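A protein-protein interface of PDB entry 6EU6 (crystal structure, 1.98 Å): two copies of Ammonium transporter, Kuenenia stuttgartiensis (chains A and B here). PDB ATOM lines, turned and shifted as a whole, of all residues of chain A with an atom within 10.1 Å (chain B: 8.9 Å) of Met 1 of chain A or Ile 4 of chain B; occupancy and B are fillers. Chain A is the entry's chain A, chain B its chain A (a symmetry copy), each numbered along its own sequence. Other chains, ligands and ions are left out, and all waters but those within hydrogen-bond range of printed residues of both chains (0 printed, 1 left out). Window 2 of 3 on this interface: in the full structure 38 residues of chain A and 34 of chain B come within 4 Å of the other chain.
Ile 4 of chain B touches Met 1 of chain A. Ile 4 of chain B touches Ile 4 of chain A. Ile 8 of chain A touches Ile 4 of chain B. Ile 8 of chain A touches Ile 8 of chain B. Ser 232 of chain A touches Asn 7 of chain B (CA to OD1, 3.8 Å). Val 233 of chain A touches His 10 of chain B (CG1 to NE2, 3.6 Å).
NE2 of Gln 5 of chain A lies within hydrogen-bond range of OD1 of Asn 9 of chain A (2.9 Å). NH1 of Arg 230 of chain A sits close to NE2 of Gln 5 of chain A, 3.2 Å away. ND2 of Asn 3 of chain A sits close to N of Met 1 of chain A (3.2 Å). The side-chain amide oxygen (OD1) of Asn 9 of chain A is in hydrogen-bond range of the backbone NH (N) of Val 231 of chain A (3.0 Å). The side-chain amide nitrogen (NE2) of Gln 5 of chain A lies within hydrogen-bond range of the backbone carbonyl oxygen (O) of Val 231 of chain A (3.1 Å).
Met 1 of chain A touches one residue of chain B. Of the printed residues of chain B, Ile 4 of chain A touches Ile 4 (3.999 Å). Printed residues of chain B within 4 Å of Gln 5 of chain A: Asn 7 (2.8 Å). Asn 9 of chain A touches none of the printed residues of chain B. Of the printed residues of chain A, Ile 4 of chain B touches Met 1, Ile 4 and Ile 8. Of chain A, only Gln 5 (2.8 Å), Val 231 (3.3 Å) and Ser 232 (3.8 Å) come within 4 Å of Asn 7 of chain B. The nearest residue of chain B that does not touch Met 1 of chain A is Met 1 of chain B (7.1 Å). The nearest printed residue of chain B that does not touch Gln 5 of chain A is Ile 4 of chain B (4.01 Å).
Of the 13 printed residues of chain A, 7 touch a printed residue of chain B. Hydrophobic or aromatic side chains of chain A within 4 Å of the printed part of chain B: Ile 4, Ile 8, Val 231 and Val 233. Along chain A the printed residues that touch a printed residue of chain B span positions 1 to 233. Of the 13 printed residues of chain B, 4 touch a printed residue of chain A. Printed residues of chain B that touch a printed residue of chain A: Ile 4, Asn 7, Ile 8 and His 10.
Met 1 of chain A touches Ile 4 of chain B, but with the chains exchanged Ile 4 of chain A does not touch Met 1 of chain B (7.8 Å). Ile 4 of chain B touches its own counterpart, Ile 4 of chain A. Ile 8 of chain B touches its own counterpart, Ile 8 of chain A. Val 231 of chain A touches Asn 7 of chain B, but with the chains exchanged Asn 7 of chain A does not touch Val 231 of chain B (12.0 Å). Positions printed for both chains: 1, 2, 3, 4, 5, 6, 7, 8, 9, 230 and 231. Of the 8 pairs that touch across the chains among the printed residues, 2 have their exchanged pair printed and touching as well.
OE1 of Gln 5 of chain A sits at hydrogen-bond distance from ND2 of Asn 7 of chain B (2.8 Å). ND2 of Asn 7 of chain B sits at hydrogen-bond distance from O of Val 231 of chain A, at 3.5 Å.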
ATOM      1  N   MET A   1      10.125 -38.070   4.111  1.00  0.00           N
ATOM      2  CA  MET A   1       9.085 -36.964   4.162  1.00  0.00           C
ATOM      3  C   MET A   1       8.429 -36.915   5.567  1.00  0.00           C
ATOM      4  O   MET A   1       8.692 -36.023   6.393  1.00  0.00           O
ATOM      5  CB  MET A   1       8.052 -37.136   3.060  1.00  0.00           C
ATOM      6  CG  MET A   1       8.434 -38.134   1.965  1.00  0.00           C
ATOM      7  SD  MET A   1       7.032 -38.698   0.983  1.00  0.00           S
ATOM      8  CE  MET A   1       6.179 -39.786   2.142  1.00  0.00           C
ATOM      9  N   GLU A   2       7.634 -37.925   5.843  1.00  0.00           N
ATOM     10  CA  GLU A   2       7.072 -38.164   7.134  1.00  0.00           C
ATOM     11  C   GLU A   2       8.266 -38.727   7.957  1.00  0.00           C
ATOM     12  O   GLU A   2       8.395 -38.438   9.146  1.00  0.00           O
ATOM     13  CB  GLU A   2       5.864 -39.152   7.083  1.00  0.00           C
ATOM     14  CG  GLU A   2       4.836 -38.962   5.936  1.00  0.00           C
ATOM     15  CD  GLU A   2       3.461 -38.432   6.374  1.00  0.00           C
ATOM     16  OE1 GLU A   2       3.426 -37.492   7.199  1.00  0.00           O
ATOM     17  OE2 GLU A   2       2.411 -38.940   5.873  1.00  0.00           O
ATOM     18  N   ASN A   3       9.146 -39.489   7.305  1.00  0.00           N
ATOM     19  CA  ASN A   3      10.306 -40.076   7.976  1.00  0.00           C
ATOM     20  C   ASN A   3      11.282 -39.004   8.422  1.00  0.00           C
ATOM     21  O   ASN A   3      11.847 -39.104   9.459  1.00  0.00           O
ATOM     22  CB  ASN A   3      11.019 -41.213   7.194  1.00  0.00           C
ATOM     23  CG  ASN A   3      10.584 -41.307   5.740  1.00  0.00           C
ATOM     24  OD1 ASN A   3       9.477 -41.786   5.423  1.00  0.00           O
ATOM     25  ND2 ASN A   3      11.453 -40.847   4.836  1.00  0.00           N
ATOM     26  N   ILE A   4      11.439 -37.948   7.666  1.00  0.00           N
ATOM     27  CA  ILE A   4      12.253 -36.837   8.109  1.00  0.00           C
ATOM     28  C   ILE A   4      11.625 -36.100   9.297  1.00  0.00           C
ATOM     29  O   ILE A   4      12.372 -35.755  10.241  1.00  0.00           O
ATOM     30  CB  ILE A   4      12.559 -35.892   6.953  1.00  0.00           C
ATOM     31  CG1 ILE A   4      13.515 -36.617   6.008  1.00  0.00           C
ATOM     32  CG2 ILE A   4      13.221 -34.625   7.430  1.00  0.00           C
ATOM     33  CD1 ILE A   4      13.899 -35.807   4.808  1.00  0.00           C
ATOM     34  N   GLN A   5      10.303 -35.823   9.263  1.00  0.00           N
ATOM     35  CA  GLN A   5       9.613 -35.247  10.424  1.00  0.00           C
ATOM     36  C   GLN A   5       9.745 -36.137  11.694  1.00  0.00           C
ATOM     37  O   GLN A   5       9.928 -35.628  12.811  1.00  0.00           O
ATOM     38  CB  GLN A   5       8.140 -34.930  10.120  1.00  0.00           C
ATOM     39  CG  GLN A   5       7.414 -34.180  11.293  1.00  0.00           C
ATOM     40  CD  GLN A   5       7.813 -32.697  11.611  1.00  0.00           C
ATOM     41  OE1 GLN A   5       7.975 -31.807  10.730  1.00  0.00           O
ATOM     42  NE2 GLN A   5       7.945 -32.422  12.898  1.00  0.00           N
ATOM     43  N   ILE A   6       9.689 -37.451  11.519  1.00  0.00           N
ATOM     44  CA  ILE A   6       9.874 -38.359  12.648  1.00  0.00           C
ATOM     45  C   ILE A   6      11.281 -38.196  13.235  1.00  0.00           C
ATOM     46  O   ILE A   6      11.432 -38.173  14.463  1.00  0.00           O
ATOM     47  CB  ILE A   6       9.657 -39.814  12.256  1.00  0.00           C
ATOM     48  CG1 ILE A   6       8.145 -40.098  12.061  1.00  0.00           C
ATOM     49  CG2 ILE A   6      10.200 -40.741  13.334  1.00  0.00           C
ATOM     50  CD1 ILE A   6       7.841 -41.475  11.457  1.00  0.00           C
ATOM     51  N   ASN A   7      12.293 -38.057  12.367  1.00  0.00           N
ATOM     52  CA  ASN A   7      13.676 -37.818  12.799  1.00  0.00           C
ATOM     53  C   ASN A   7      13.854 -36.511  13.579  1.00  0.00           C
ATOM     54  O   ASN A   7      14.532 -36.488  14.576  1.00  0.00           O
ATOM     55  CB  ASN A   7      14.649 -37.773  11.628  1.00  0.00           C
ATOM     56  CG  ASN A   7      14.957 -39.147  11.109  1.00  0.00           C
ATOM     57  OD1 ASN A   7      14.622 -40.111  11.766  1.00  0.00           O
ATOM     58  ND2 ASN A   7      15.598 -39.231   9.928  1.00  0.00           N
ATOM     59  N   ILE A   8      13.224 -35.456  13.113  1.00  0.00           N
ATOM     60  CA  ILE A   8      13.260 -34.140  13.780  1.00  0.00           C
ATOM     61  C   ILE A   8      12.585 -34.273  15.171  1.00  0.00           C
ATOM     62  O   ILE A   8      12.992 -33.616  16.116  1.00  0.00           O
ATOM     63  CB  ILE A   8      12.466 -33.186  12.891  1.00  0.00           C
ATOM     64  CG1 ILE A   8      13.307 -32.852  11.673  1.00  0.00           C
ATOM     65  CG2 ILE A   8      12.050 -31.942  13.585  1.00  0.00           C
ATOM     66  CD1 ILE A   8      12.490 -32.158  10.587  1.00  0.00           C
ATOM     67  N   ASN A   9      11.540 -35.093  15.248  1.00  0.00           N
ATOM     68  CA  ASN A   9      10.749 -35.232  16.446  1.00  0.00           C
ATOM     69  C   ASN A   9      11.549 -35.989  17.497  1.00  0.00           C
ATOM     70  O   ASN A   9      11.563 -35.604  18.681  1.00  0.00           O
ATOM     71  CB  ASN A   9       9.445 -35.961  16.169  1.00  0.00           C
ATOM     72  CG  ASN A   9       8.441 -35.120  15.466  1.00  0.00           C
ATOM     73  OD1 ASN A   9       8.548 -33.920  15.267  1.00  0.00           O
ATOM     74  ND2 ASN A   9       7.428 -35.779  15.019  1.00  0.00           N
ATOM     75  N   ARG A 230       6.821 -33.351  19.494  1.00  0.00           N
ATOM     76  CA  ARG A 230       7.019 -33.134  18.064  1.00  0.00           C
ATOM     77  C   ARG A 230       7.482 -31.698  17.901  1.00  0.00           C
ATOM     78  O   ARG A 230       7.312 -30.886  18.805  1.00  0.00           O
ATOM     79  CB  ARG A 230       5.741 -33.352  17.244  1.00  0.00           C
ATOM     80  CG  ARG A 230       4.771 -32.181  17.282  1.00  0.00           C
ATOM     81  CD  ARG A 230       3.589 -32.425  16.352  1.00  0.00           C
ATOM     82  NE  ARG A 230       3.983 -33.453  15.416  1.00  0.00           N
ATOM     83  CZ  ARG A 230       4.630 -33.224  14.274  1.00  0.00           C
ATOM     84  NH1 ARG A 230       4.908 -31.959  13.874  1.00  0.00           N
ATOM     85  NH2 ARG A 230       4.972 -34.272  13.542  1.00  0.00           N
ATOM     86  N   VAL A 231       8.082 -31.391  16.763  1.00  0.00           N
ATOM     87  CA  VAL A 231       8.510 -30.039  16.513  1.00  0.00           C
ATOM     88  C   VAL A 231       7.494 -29.390  15.661  1.00  0.00           C
ATOM     89  O   VAL A 231       7.184 -29.898  14.614  1.00  0.00           O
ATOM     90  CB  VAL A 231       9.843 -30.024  15.746  1.00  0.00           C
ATOM     91  CG1 VAL A 231      10.325 -28.604  15.594  1.00  0.00           C
ATOM     92  CG2 VAL A 231      10.882 -30.902  16.442  1.00  0.00           C
ATOM     93  N   SER A 232       6.984 -28.255  16.101  1.00  0.00           N
ATOM     94  CA  SER A 232       6.112 -27.372  15.289  1.00  0.00           C
ATOM     95  C   SER A 232       6.451 -25.957  15.703  1.00  0.00           C
ATOM     96  O   SER A 232       7.177 -25.722  16.657  1.00  0.00           O
ATOM     97  CB  SER A 232       4.619 -27.603  15.533  1.00  0.00           C
ATOM     98  OG  SER A 232       4.261 -27.722  16.908  1.00  0.00           O
ATOM     99  N   VAL A 233       5.863 -25.027  15.023  1.00  0.00           N
ATOM    100  CA  VAL A 233       5.830 -23.610  15.414  1.00  0.00           C
ATOM    101  C   VAL A 233       5.407 -23.387  16.887  1.00  0.00           C
ATOM    102  O   VAL A 233       5.826 -22.440  17.580  1.00  0.00           O
ATOM    103  CB  VAL A 233       4.908 -22.871  14.398  1.00  0.00           C
ATOM    104  CG1 VAL A 233       5.325 -23.238  12.964  1.00  0.00           C
ATOM    105  CG2 VAL A 233       3.462 -23.281  14.536  1.00  0.00           C
ATOM    106  N   MET B   1       7.785 -29.751   3.197  1.00  0.00           N
ATOM    107  CA  MET B   1       9.062 -29.531   2.405  1.00  0.00           C
ATOM    108  C   MET B   1       9.775 -28.241   2.892  1.00  0.00           C
ATOM    109  O   MET B   1      10.804 -28.274   3.589  1.00  0.00           O
ATOM    110  CB  MET B   1       8.777 -29.490   0.912  1.00  0.00           C
ATOM    111  CG  MET B   1       7.391 -29.997   0.504  1.00  0.00           C
ATOM    112  SD  MET B   1       6.890 -29.474  -1.147  1.00  0.00           S
ATOM    113  CE  MET B   1       6.543 -27.721  -0.893  1.00  0.00           C
ATOM    114  N   GLU B   2       9.168 -27.119   2.575  1.00  0.00           N
ATOM    115  CA  GLU B   2       9.556 -25.837   3.073  1.00  0.00           C
ATOM    116  C   GLU B   2       9.040 -25.840   4.540  1.00  0.00           C
ATOM    117  O   GLU B   2       9.691 -25.295   5.431  1.00  0.00           O
ATOM    118  CB  GLU B   2       8.956 -24.667   2.231  1.00  0.00           C
ATOM    119  CG  GLU B   2       8.980 -24.815   0.686  1.00  0.00           C
ATOM    120  CD  GLU B   2       9.962 -23.885  -0.044  1.00  0.00           C
ATOM    121  OE1 GLU B   2      11.110 -23.746   0.434  1.00  0.00           O
ATOM    122  OE2 GLU B   2       9.593 -23.308  -1.113  1.00  0.00           O
ATOM    123  N   ASN B   3       7.898 -26.487   4.781  1.00  0.00           N
ATOM    124  CA  ASN B   3       7.315 -26.553   6.121  1.00  0.00           C
ATOM    125  C   ASN B   3       8.190 -27.362   7.060  1.00  0.00           C
ATOM    126  O   ASN B   3       8.327 -27.025   8.188  1.00  0.00           O
ATOM    127  CB  ASN B   3       5.832 -27.013   6.176  1.00  0.00           C
ATOM    128  CG  ASN B   3       5.340 -27.614   4.870  1.00  0.00           C
ATOM    129  OD1 ASN B   3       5.077 -26.896   3.884  1.00  0.00           O
ATOM    130  ND2 ASN B   3       5.209 -28.943   4.846  1.00  0.00           N
ATOM    131  N   ILE B   4       8.829 -28.399   6.582  1.00  0.00           N
ATOM    132  CA  ILE B   4       9.780 -29.121   7.399  1.00  0.00           C
ATOM    133  C   ILE B   4      11.025 -28.285   7.711  1.00  0.00           C
ATOM    134  O   ILE B   4      11.483 -28.317   8.877  1.00  0.00           O
ATOM    135  CB  ILE B   4      10.139 -30.458   6.762  1.00  0.00           C
ATOM    136  CG1 ILE B   4       8.907 -31.357   6.853  1.00  0.00           C
ATOM    137  CG2 ILE B   4      11.279 -31.130   7.483  1.00  0.00           C
ATOM    138  CD1 ILE B   4       9.109 -32.713   6.251  1.00  0.00           C
ATOM    139  N   GLN B   5      11.598 -27.577   6.712  1.00  0.00           N
ATOM    140  CA  GLN B   5      12.705 -26.649   6.972  1.00  0.00           C
ATOM    141  C   GLN B   5      12.326 -25.546   8.001  1.00  0.00           C
ATOM    142  O   GLN B   5      13.135 -25.177   8.866  1.00  0.00           O
ATOM    143  CB  GLN B   5      13.258 -26.033   5.676  1.00  0.00           C
ATOM    144  CG  GLN B   5      14.534 -25.149   5.906  1.00  0.00           C
ATOM    145  CD  GLN B   5      15.879 -25.846   6.312  1.00  0.00           C
ATOM    146  OE1 GLN B   5      16.323 -26.893   5.763  1.00  0.00           O
ATOM    147  NE2 GLN B   5      16.553 -25.236   7.273  1.00  0.00           N
ATOM    148  N   ILE B   6      11.097 -25.051   7.930  1.00  0.00           N
ATOM    149  CA  ILE B   6      10.636 -24.063   8.901  1.00  0.00           C
ATOM    150  C   ILE B   6      10.635 -24.665  10.311  1.00  0.00           C
ATOM    151  O   ILE B   6      11.055 -23.994  11.262  1.00  0.00           O
ATOM    152  CB  ILE B   6       9.244 -23.541   8.574  1.00  0.00           C
ATOM    153  CG1 ILE B   6       9.303 -22.571   7.366  1.00  0.00           C
ATOM    154  CG2 ILE B   6       8.657 -22.806   9.771  1.00  0.00           C
ATOM    155  CD1 ILE B   6       7.927 -22.162   6.825  1.00  0.00           C
ATOM    156  N   ASN B   7      10.193 -25.924  10.437  1.00  0.00           N
ATOM    157  CA  ASN B   7      10.209 -26.641  11.718  1.00  0.00           C
ATOM    158  C   ASN B   7      11.617 -26.828  12.294  1.00  0.00           C
ATOM    159  O   ASN B   7      11.822 -26.642  13.467  1.00  0.00           O
ATOM    160  CB  ASN B   7       9.584 -28.027  11.615  1.00  0.00           C
ATOM    161  CG  ASN B   7       8.086 -27.959  11.574  1.00  0.00           C
ATOM    162  OD1 ASN B   7       7.539 -26.910  11.849  1.00  0.00           O
ATOM    163  ND2 ASN B   7       7.427 -29.081  11.232  1.00  0.00           N
ATOM    164  N   ILE B   8      12.561 -27.175  11.446  1.00  0.00           N
ATOM    165  CA  ILE B   8      13.971 -27.346  11.841  1.00  0.00           C
ATOM    166  C   ILE B   8      14.520 -25.975  12.317  1.00  0.00           C
ATOM    167  O   ILE B   8      15.345 -25.922  13.216  1.00  0.00           O
ATOM    168  CB  ILE B   8      14.714 -27.812  10.591  1.00  0.00           C
ATOM    169  CG1 ILE B   8      14.366 -29.267  10.338  1.00  0.00           C
ATOM    170  CG2 ILE B   8      16.185 -27.644  10.682  1.00  0.00           C
ATOM    171  CD1 ILE B   8      14.810 -29.731   8.954  1.00  0.00           C
ATOM    172  N   ASN B   9      14.077 -24.900  11.670  1.00  0.00           N
ATOM    173  CA  ASN B   9      14.581 -23.575  11.930  1.00  0.00           C
ATOM    174  C   ASN B   9      14.071 -23.095  13.283  1.00  0.00           C
ATOM    175  O   ASN B   9      14.836 -22.522  14.080  1.00  0.00           O
ATOM    176  CB  ASN B   9      14.157 -22.597  10.847  1.00  0.00           C
ATOM    177  CG  ASN B   9      14.917 -22.761   9.580  1.00  0.00           C
ATOM    178  OD1 ASN B   9      15.898 -23.476   9.439  1.00  0.00           O
ATOM    179  ND2 ASN B   9      14.423 -22.108   8.585  1.00  0.00           N
ATOM    180  N   HIS B  10      12.819 -23.390  13.587  1.00  0.00           N
ATOM    181  CA  HIS B  10      12.287 -23.204  14.941  1.00  0.00           C
ATOM    182  C   HIS B  10      13.051 -23.960  15.998  1.00  0.00           C
ATOM    183  O   HIS B  10      13.408 -23.416  17.012  1.00  0.00           O
ATOM    184  CB  HIS B  10      10.818 -23.622  15.058  1.00  0.00           C
ATOM    185  CG  HIS B  10       9.857 -22.617  14.537  1.00  0.00           C
ATOM    186  ND1 HIS B  10       9.451 -21.536  15.271  1.00  0.00           N
ATOM    187  CD2 HIS B  10       9.139 -22.575  13.395  1.00  0.00           C
ATOM    188  CE1 HIS B  10       8.584 -20.829  14.585  1.00  0.00           C
ATOM    189  NE2 HIS B  10       8.389 -21.428  13.441  1.00  0.00           N
ATOM    190  N   LEU B  11      13.292 -25.230  15.746  1.00  0.00           N
ATOM    191  CA  LEU B  11      13.986 -26.049  16.676  1.00  0.00           C
ATOM    192  C   LEU B  11      15.343 -25.435  17.028  1.00  0.00           C
ATOM    193  O   LEU B  11      15.701 -25.361  18.228  1.00  0.00           O
ATOM    194  CB  LEU B  11      14.147 -27.451  16.121  1.00  0.00           C
ATOM    195  CG  LEU B  11      14.946 -28.462  16.956  1.00  0.00           C
ATOM    196  CD1 LEU B  11      14.398 -28.551  18.371  1.00  0.00           C
ATOM    197  CD2 LEU B  11      14.911 -29.825  16.253  1.00  0.00           C
ATOM    198  N   ARG B 230      18.357 -19.938  11.056  1.00  0.00           N
ATOM    199  CA  ARG B 230      17.992 -21.064  10.201  1.00  0.00           C
ATOM    200  C   ARG B 230      19.107 -22.085  10.326  1.00  0.00           C
ATOM    201  O   ARG B 230      20.202 -21.756  10.769  1.00  0.00           O
ATOM    202  CB  ARG B 230      17.828 -20.668   8.728  1.00  0.00           C
ATOM    203  CG  ARG B 230      19.141 -20.529   7.973  1.00  0.00           C
ATOM    204  CD  ARG B 230      18.889 -20.252   6.495  1.00  0.00           C
ATOM    205  NE  ARG B 230      17.532 -20.652   6.207  1.00  0.00           N
ATOM    206  CZ  ARG B 230      17.165 -21.890   5.875  1.00  0.00           C
ATOM    207  NH1 ARG B 230      18.089 -22.869   5.715  1.00  0.00           N
ATOM    208  NH2 ARG B 230      15.876 -22.118   5.691  1.00  0.00           N
ATOM    209  N   VAL B 231      18.823 -23.324   9.957  1.00  0.00           N
ATOM    210  CA  VAL B 231      19.841 -24.342  10.002  1.00  0.00           C
ATOM    211  C   VAL B 231      20.378 -24.510   8.638  1.00  0.00           C
ATOM    212  O   VAL B 231      19.627 -24.754   7.729  1.00  0.00           O
ATOM    213  CB  VAL B 231      19.242 -25.690  10.439  1.00  0.00           C
ATOM    214  CG1 VAL B 231      20.342 -26.711  10.586  1.00  0.00           C
ATOM    215  CG2 VAL B 231      18.437 -25.536  11.729  1.00  0.00           C
